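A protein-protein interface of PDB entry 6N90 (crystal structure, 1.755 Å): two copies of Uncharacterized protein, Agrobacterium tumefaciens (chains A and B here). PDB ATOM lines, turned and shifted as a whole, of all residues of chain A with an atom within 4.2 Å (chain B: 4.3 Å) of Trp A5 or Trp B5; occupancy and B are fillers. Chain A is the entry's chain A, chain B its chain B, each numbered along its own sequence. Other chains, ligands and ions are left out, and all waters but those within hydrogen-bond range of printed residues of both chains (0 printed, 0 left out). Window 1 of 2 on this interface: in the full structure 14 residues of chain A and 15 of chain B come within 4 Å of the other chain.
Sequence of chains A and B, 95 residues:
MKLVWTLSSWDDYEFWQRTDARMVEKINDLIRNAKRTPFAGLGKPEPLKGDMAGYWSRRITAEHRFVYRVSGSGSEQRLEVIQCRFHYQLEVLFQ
O of Leu A3 is in hydrogen-bond range of N of Trp B5, 2.8 Å away.
The backbone NH (N) of Trp A5 is in hydrogen-bond range of the backbone carbonyl oxygen (O) of Leu B3, at 2.7 Å.
NE1 of Trp B5 sits close to NE1 of Trp A5 (3.5 Å).
O of Val A4 lies within hydrogen-bond range of N of Val A81, 2.8 Å away.
The backbone carbonyl oxygen of Val B4 is in hydrogen-bond range of the backbone NH of Val B81, at 2.7 Å.
Among the printed residues, pairs that only touch across the chains: Lys A2 with Trp B5 (3.3 Å), Val A4 with Leu B3 (3.4 Å), Leu A3 with Trp B10 (3.4 Å), Leu A3 with Val B4 (3.4 Å), Tyr A13 with Trp B10 (3.4 Å), Trp A5 with Lys B2 (3.4 Å), Trp A10 with Leu B3 (3.4 Å), Trp A10 with Tyr B13 (3.5 Å), Leu A3 with Leu B3 (3.5 Å), Trp A10 with Trp B5 (3.8 Å), Trp A5 with Trp B10 (3.8 Å), Lys A2 with Val B4 (3.9 Å), Trp A10 with Ile B31 (3.9 Å) and Tyr A13 with Tyr B13 (3.98 Å).
Of the printed residues of chain B, Leu A3 touches Leu B3, Val B4, Trp B5 and Trp B10.
Of the printed residues of chain B, Val A4 touches Leu B3 (3.4 Å).
Ile A31 touches none of the printed residues of chain B.
Of chain A, only Lys A2 (3.3 Å), Leu A3 (2.8 Å), Trp A5 (3.5 Å) and Trp A10 (3.8 Å) come within 4 Å of Trp B5.
Cys B84 touches none of the printed residues of chain A.
The nearest printed residue of chain B that does not touch Trp A5 is Val B4 (5.0 Å).
The nearest printed residue of chain A that does not touch Trp B5 is Val A4 (5.0 Å).
The nearest printed residue of chain B that does not touch Lys A2 is Thr B6 (4.6 Å).
Hydrophobic or aromatic side chains of chain B within 4 Å of the printed part of chain A: Leu B3, Val B4, Trp B5, Trp B10, Tyr B13 and Ile B31.
Along chain B the printed residues that touch a printed residue of chain A span positions 2 to 31.
Hydrophobic or aromatic side chains of chain A within 4 Å of the printed part of chain B: Leu A3, Trp A5, Trp A10 and Tyr A13.
Among the printed residues, 17 pairs touch across the chains.
Leu A3 touches Val B4, and with the chains exchanged Val A4 touches Leu B3.
Trp A10 touches Tyr B13, and with the chains exchanged Tyr A13 touches Trp B10.
Trp A10 touches Ile B31, but with the chains exchanged Ile A31 does not touch Trp B10 (4.04 Å).
Tyr B13 touches its own counterpart, Tyr A13.
Positions printed for both chains: 2, 3, 4, 5, 6, 9, 10, 13, 31 and 81.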
ATOM      1  N   LYS A   2       5.493  21.062 -20.732  1.00  0.00           N
ATOM      2  CA  LYS A   2       5.422  22.419 -21.254  1.00  0.00           C
ATOM      3  C   LYS A   2       6.667  22.760 -22.064  1.00  0.00           C
ATOM      4  O   LYS A   2       7.731  22.191 -21.856  1.00  0.00           O
ATOM      5  CB  LYS A   2       5.214  23.416 -20.112  1.00  0.00           C
ATOM      6  CG  LYS A   2       3.954  23.104 -19.315  1.00  0.00           C
ATOM      7  CD  LYS A   2       3.462  24.237 -18.420  1.00  0.00           C
ATOM      8  CE  LYS A   2       2.064  23.873 -17.903  1.00  0.00           C
ATOM      9  NZ  LYS A   2       1.403  24.966 -17.142  1.00  0.00           N
ATOM     10  N   LEU A   3       6.506  23.671 -23.018  1.00  0.00           N
ATOM     11  CA  LEU A   3       7.602  24.163 -23.829  1.00  0.00           C
ATOM     12  C   LEU A   3       7.797  25.629 -23.464  1.00  0.00           C
ATOM     13  O   LEU A   3       6.885  26.425 -23.613  1.00  0.00           O
ATOM     14  CB  LEU A   3       7.295  23.989 -25.331  1.00  0.00           C
ATOM     15  CG  LEU A   3       8.302  24.574 -26.305  1.00  0.00           C
ATOM     16  CD1 LEU A   3       9.633  23.920 -26.157  1.00  0.00           C
ATOM     17  CD2 LEU A   3       7.784  24.341 -27.735  1.00  0.00           C
ATOM     18  N   VAL A   4       8.969  25.974 -22.941  1.00  0.00           N
ATOM     19  CA  VAL A   4       9.255  27.331 -22.475  1.00  0.00           C
ATOM     20  C   VAL A   4      10.341  28.029 -23.299  1.00  0.00           C
ATOM     21  O   VAL A   4      11.443  27.524 -23.449  1.00  0.00           O
ATOM     22  CB  VAL A   4       9.694  27.326 -20.989  1.00  0.00           C
ATOM     23  CG1 VAL A   4       9.871  28.749 -20.530  1.00  0.00           C
ATOM     24  CG2 VAL A   4       8.668  26.574 -20.149  1.00  0.00           C
ATOM     25  N   TRP A   5      10.004  29.188 -23.864  1.00  0.00           N
ATOM     26  CA  TRP A   5      10.982  30.019 -24.557  1.00  0.00           C
ATOM     27  C   TRP A   5      11.335  31.257 -23.755  1.00  0.00           C
ATOM     28  O   TRP A   5      10.497  31.836 -23.092  1.00  0.00           O
ATOM     29  CB  TRP A   5      10.441  30.507 -25.896  1.00  0.00           C
ATOM     30  CG  TRP A   5       9.944  29.439 -26.780  1.00  0.00           C
ATOM     31  CD1 TRP A   5       8.718  28.822 -26.722  1.00  0.00           C
ATOM     32  CD2 TRP A   5      10.626  28.883 -27.902  1.00  0.00           C
ATOM     33  NE1 TRP A   5       8.605  27.908 -27.748  1.00  0.00           N
ATOM     34  CE2 TRP A   5       9.770  27.918 -28.478  1.00  0.00           C
ATOM     35  CE3 TRP A   5      11.889  29.084 -28.472  1.00  0.00           C
ATOM     36  CZ2 TRP A   5      10.132  27.174 -29.604  1.00  0.00           C
ATOM     37  CZ3 TRP A   5      12.237  28.345 -29.595  1.00  0.00           C
ATOM     38  CH2 TRP A   5      11.370  27.388 -30.134  1.00  0.00           C
ATOM     39  N   THR A   6      12.556  31.725 -23.918  1.00  0.00           N
ATOM     40  CA  THR A   6      12.926  33.038 -23.407  1.00  0.00           C
ATOM     41  C   THR A   6      12.635  34.129 -24.428  1.00  0.00           C
ATOM     42  O   THR A   6      12.239  33.836 -25.560  1.00  0.00           O
ATOM     43  CB  THR A   6      14.405  33.073 -23.036  1.00  0.00           C
ATOM     44  OG1 THR A   6      15.188  32.845 -24.213  1.00  0.00           O
ATOM     45  CG2 THR A   6      14.695  31.978 -22.010  1.00  0.00           C
ATOM     46  N   SER A   9      15.310  33.434 -27.210  1.00  0.00           N
ATOM     47  CA  SER A   9      15.183  32.226 -28.018  1.00  0.00           C
ATOM     48  C   SER A   9      13.929  32.326 -28.911  1.00  0.00           C
ATOM     49  O   SER A   9      13.944  31.883 -30.068  1.00  0.00           O
ATOM     50  CB  SER A   9      15.171  30.944 -27.156  1.00  0.00           C
ATOM     51  OG  SER A   9      14.013  30.806 -26.346  1.00  0.00           O
ATOM     52  N   TRP A  10      12.863  32.940 -28.408  1.00  0.00           N
ATOM     53  CA  TRP A  10      11.676  33.126 -29.258  1.00  0.00           C
ATOM     54  C   TRP A  10      11.967  34.104 -30.398  1.00  0.00           C
ATOM     55  O   TRP A  10      11.530  33.904 -31.542  1.00  0.00           O
ATOM     56  CB  TRP A  10      10.475  33.612 -28.437  1.00  0.00           C
ATOM     57  CG  TRP A  10       9.201  33.681 -29.268  1.00  0.00           C
ATOM     58  CD1 TRP A  10       8.530  34.825 -29.666  1.00  0.00           C
ATOM     59  CD2 TRP A  10       8.468  32.573 -29.830  1.00  0.00           C
ATOM     60  NE1 TRP A  10       7.429  34.481 -30.435  1.00  0.00           N
ATOM     61  CE2 TRP A  10       7.368  33.114 -30.544  1.00  0.00           C
ATOM     62  CE3 TRP A  10       8.624  31.181 -29.788  1.00  0.00           C
ATOM     63  CZ2 TRP A  10       6.433  32.308 -31.193  1.00  0.00           C
ATOM     64  CZ3 TRP A  10       7.695  30.379 -30.442  1.00  0.00           C
ATOM     65  CH2 TRP A  10       6.616  30.948 -31.147  1.00  0.00           C
ATOM     66  N   TYR A  13      13.808  32.198 -32.975  1.00  0.00           N
ATOM     67  CA  TYR A  13      12.889  31.280 -33.665  1.00  0.00           C
ATOM     68  C   TYR A  13      12.057  32.051 -34.680  1.00  0.00           C
ATOM     69  O   TYR A  13      11.861  31.582 -35.791  1.00  0.00           O
ATOM     70  CB  TYR A  13      11.981  30.587 -32.662  1.00  0.00           C
ATOM     71  CG  TYR A  13      11.061  29.493 -33.189  1.00  0.00           C
ATOM     72  CD1 TYR A  13      11.558  28.251 -33.586  1.00  0.00           C
ATOM     73  CD2 TYR A  13       9.684  29.678 -33.166  1.00  0.00           C
ATOM     74  CE1 TYR A  13      10.687  27.230 -34.007  1.00  0.00           C
ATOM     75  CE2 TYR A  13       8.811  28.685 -33.590  1.00  0.00           C
ATOM     76  CZ  TYR A  13       9.311  27.472 -34.020  1.00  0.00           C
ATOM     77  OH  TYR A  13       8.423  26.491 -34.424  1.00  0.00           O
ATOM     78  N   ILE A  31      12.836  19.711 -30.892  1.00  0.00           N
ATOM     79  CA  ILE A  31      11.898  19.852 -29.775  1.00  0.00           C
ATOM     80  C   ILE A  31      11.115  18.550 -29.527  1.00  0.00           C
ATOM     81  O   ILE A  31      11.104  18.007 -28.386  1.00  0.00           O
ATOM     82  CB  ILE A  31      10.922  21.026 -30.031  1.00  0.00           C
ATOM     83  CG1 ILE A  31      11.672  22.354 -29.975  1.00  0.00           C
ATOM     84  CG2 ILE A  31       9.737  21.020 -29.024  1.00  0.00           C
ATOM     85  CD1 ILE A  31      10.858  23.554 -30.330  1.00  0.00           C
ATOM     86  N   VAL A  81      13.841  26.194 -23.797  1.00  0.00           N
ATOM     87  CA  VAL A  81      14.772  26.508 -24.874  1.00  0.00           C
ATOM     88  C   VAL A  81      15.517  27.800 -24.560  1.00  0.00           C
ATOM     89  O   VAL A  81      14.901  28.854 -24.398  1.00  0.00           O
ATOM     90  CB  VAL A  81      14.056  26.663 -26.221  1.00  0.00           C
ATOM     91  CG1 VAL A  81      15.083  26.973 -27.355  1.00  0.00           C
ATOM     92  CG2 VAL A  81      13.219  25.431 -26.504  1.00  0.00           C
ATOM     93  N   LYS B   2       8.752  35.234 -20.318  1.00  0.00           N
ATOM     94  CA  LYS B   2       8.870  33.914 -20.927  1.00  0.00           C
ATOM     95  C   LYS B   2       7.564  33.438 -21.578  1.00  0.00           C
ATOM     96  O   LYS B   2       6.450  33.773 -21.145  1.00  0.00           O
ATOM     97  CB  LYS B   2       9.355  32.894 -19.902  1.00  0.00           C
ATOM     98  CG  LYS B   2      10.825  33.089 -19.533  1.00  0.00           C
ATOM     99  CD  LYS B   2      11.271  32.161 -18.447  1.00  0.00           C
ATOM    100  CE  LYS B   2      12.634  32.576 -17.914  1.00  0.00           C
ATOM    101  NZ  LYS B   2      12.959  31.836 -16.659  1.00  0.00           N
ATOM    102  N   LEU B   3       7.735  32.671 -22.647  1.00  0.00           N
ATOM    103  CA  LEU B   3       6.624  32.188 -23.463  1.00  0.00           C
ATOM    104  C   LEU B   3       6.454  30.704 -23.223  1.00  0.00           C
ATOM    105  O   LEU B   3       7.385  29.935 -23.489  1.00  0.00           O
ATOM    106  CB  LEU B   3       6.886  32.469 -24.943  1.00  0.00           C
ATOM    107  CG  LEU B   3       5.745  32.091 -25.879  1.00  0.00           C
ATOM    108  CD1 LEU B   3       4.456  32.748 -25.461  1.00  0.00           C
ATOM    109  CD2 LEU B   3       6.125  32.465 -27.312  1.00  0.00           C
ATOM    110  N   VAL B   4       5.286  30.323 -22.697  1.00  0.00           N
ATOM    111  CA  VAL B   4       5.012  28.945 -22.297  1.00  0.00           C
ATOM    112  C   VAL B   4       3.886  28.328 -23.135  1.00  0.00           C
ATOM    113  O   VAL B   4       2.797  28.889 -23.263  1.00  0.00           O
ATOM    114  CB  VAL B   4       4.637  28.852 -20.806  1.00  0.00           C
ATOM    115  CG1 VAL B   4       4.497  27.382 -20.398  1.00  0.00           C
ATOM    116  CG2 VAL B   4       5.691  29.538 -19.950  1.00  0.00           C
ATOM    117  N   TRP B   5       4.167  27.168 -23.708  1.00  0.00           N
ATOM    118  CA  TRP B   5       3.153  26.406 -24.420  1.00  0.00           C
ATOM    119  C   TRP B   5       2.837  25.106 -23.704  1.00  0.00           C
ATOM    120  O   TRP B   5       3.731  24.508 -23.122  1.00  0.00           O
ATOM    121  CB  TRP B   5       3.633  26.045 -25.813  1.00  0.00           C
ATOM    122  CG  TRP B   5       4.049  27.192 -26.637  1.00  0.00           C
ATOM    123  CD1 TRP B   5       5.253  27.826 -26.619  1.00  0.00           C
ATOM    124  CD2 TRP B   5       3.270  27.824 -27.663  1.00  0.00           C
ATOM    125  NE1 TRP B   5       5.279  28.823 -27.574  1.00  0.00           N
ATOM    126  CE2 TRP B   5       4.072  28.839 -28.230  1.00  0.00           C
ATOM    127  CE3 TRP B   5       1.984  27.611 -28.173  1.00  0.00           C
ATOM    128  CZ2 TRP B   5       3.619  29.668 -29.276  1.00  0.00           C
ATOM    129  CZ3 TRP B   5       1.529  28.446 -29.240  1.00  0.00           C
ATOM    130  CH2 TRP B   5       2.342  29.456 -29.757  1.00  0.00           C
ATOM    131  N   THR B   6       1.605  24.621 -23.836  1.00  0.00           N
ATOM    132  CA  THR B   6       1.291  23.265 -23.356  1.00  0.00           C
ATOM    133  C   THR B   6       1.483  22.281 -24.495  1.00  0.00           C
ATOM    134  O   THR B   6       1.775  22.687 -25.611  1.00  0.00           O
ATOM    135  CB  THR B   6      -0.133  23.132 -22.864  1.00  0.00           C
ATOM    136  OG1 THR B   6      -1.021  23.359 -23.969  1.00  0.00           O
ATOM    137  CG2 THR B   6      -0.415  24.124 -21.734  1.00  0.00           C
ATOM    138  N   SER B   9      -1.410  23.288 -27.016  1.00  0.00           N
ATOM    139  CA  SER B   9      -1.278  24.550 -27.778  1.00  0.00           C
ATOM    140  C   SER B   9      -0.054  24.565 -28.699  1.00  0.00           C
ATOM    141  O   SER B   9      -0.095  25.182 -29.782  1.00  0.00           O
ATOM    142  CB  SER B   9      -1.239  25.749 -26.835  1.00  0.00           C
ATOM    143  OG  SER B   9      -0.021  25.810 -26.116  1.00  0.00           O
ATOM    144  N   TRP B  10       1.020  23.875 -28.327  1.00  0.00           N
ATOM    145  CA  TRP B  10       2.144  23.746 -29.263  1.00  0.00           C
ATOM    146  C   TRP B  10       1.711  22.891 -30.454  1.00  0.00           C
ATOM    147  O   TRP B  10       2.113  23.153 -31.598  1.00  0.00           O
ATOM    148  CB  TRP B  10       3.397  23.153 -28.588  1.00  0.00           C
ATOM    149  CG  TRP B  10       4.582  23.153 -29.508  1.00  0.00           C
ATOM    150  CD1 TRP B  10       5.220  22.061 -30.037  1.00  0.00           C
ATOM    151  CD2 TRP B  10       5.267  24.303 -30.016  1.00  0.00           C
ATOM    152  NE1 TRP B  10       6.265  22.468 -30.838  1.00  0.00           N
ATOM    153  CE2 TRP B  10       6.308  23.837 -30.852  1.00  0.00           C
ATOM    154  CE3 TRP B  10       5.085  25.690 -29.864  1.00  0.00           C
ATOM    155  CZ2 TRP B  10       7.174  24.705 -31.532  1.00  0.00           C
ATOM    156  CZ3 TRP B  10       5.965  26.555 -30.537  1.00  0.00           C
ATOM    157  CH2 TRP B  10       6.987  26.051 -31.362  1.00  0.00           C
ATOM    158  N   TYR B  13      -0.102  25.122 -32.745  1.00  0.00           N
ATOM    159  CA  TYR B  13       0.794  26.040 -33.439  1.00  0.00           C
ATOM    160  C   TYR B  13       1.511  25.325 -34.577  1.00  0.00           C
ATOM    161  O   TYR B  13       1.641  25.871 -35.676  1.00  0.00           O
ATOM    162  CB  TYR B  13       1.801  26.614 -32.463  1.00  0.00           C
ATOM    163  CG  TYR B  13       2.660  27.727 -32.999  1.00  0.00           C
ATOM    164  CD1 TYR B  13       2.132  28.999 -33.237  1.00  0.00           C
ATOM    165  CD2 TYR B  13       4.018  27.526 -33.190  1.00  0.00           C
ATOM    166  CE1 TYR B  13       2.948  30.041 -33.669  1.00  0.00           C
ATOM    167  CE2 TYR B  13       4.837  28.544 -33.650  1.00  0.00           C
ATOM    168  CZ  TYR B  13       4.295  29.797 -33.896  1.00  0.00           C
ATOM    169  OH  TYR B  13       5.134  30.811 -34.303  1.00  0.00           O
ATOM    170  N   ILE B  31       0.829  37.083 -29.786  1.00  0.00           N
ATOM    171  CA  ILE B  31       1.886  36.871 -28.765  1.00  0.00           C
ATOM    172  C   ILE B  31       2.683  38.163 -28.497  1.00  0.00           C
ATOM    173  O   ILE B  31       2.915  38.575 -27.343  1.00  0.00           O
ATOM    174  CB  ILE B  31       2.862  35.760 -29.212  1.00  0.00           C
ATOM    175  CG1 ILE B  31       2.167  34.397 -29.182  1.00  0.00           C
ATOM    176  CG2 ILE B  31       4.148  35.770 -28.347  1.00  0.00           C
ATOM    177  CD1 ILE B  31       2.897  33.324 -29.997  1.00  0.00           C
ATOM    178  N   VAL B  81       0.429  30.183 -23.320  1.00  0.00           N
ATOM    179  CA  VAL B  81      -0.574  29.920 -24.359  1.00  0.00           C
ATOM    180  C   VAL B  81      -1.240  28.556 -24.119  1.00  0.00           C
ATOM    181  O   VAL B  81      -0.578  27.509 -24.100  1.00  0.00           O
ATOM    182  CB  VAL B  81       0.034  29.972 -25.769  1.00  0.00           C
ATOM    183  CG1 VAL B  81      -1.078  29.821 -26.846  1.00  0.00           C
ATOM    184  CG2 VAL B  81       0.789  31.275 -25.959  1.00  0.00           C
ATOM    185  N   CYS B  84      -4.705  27.696 -29.376  1.00  0.00           N
ATOM    186  CA  CYS B  84      -4.773  28.644 -30.498  1.00  0.00           C
ATOM    187  C   CYS B  84      -5.383  28.013 -31.745  1.00  0.00           C
ATOM    188  O   CYS B  84      -5.017  28.344 -32.874  1.00  0.00           O
ATOM    189  CB  CYS B  84      -3.392  29.234 -30.818  1.00  0.00           C
ATOM    190  SG  CYS B  84      -2.067  28.100 -31.299  1.00  0.00           S
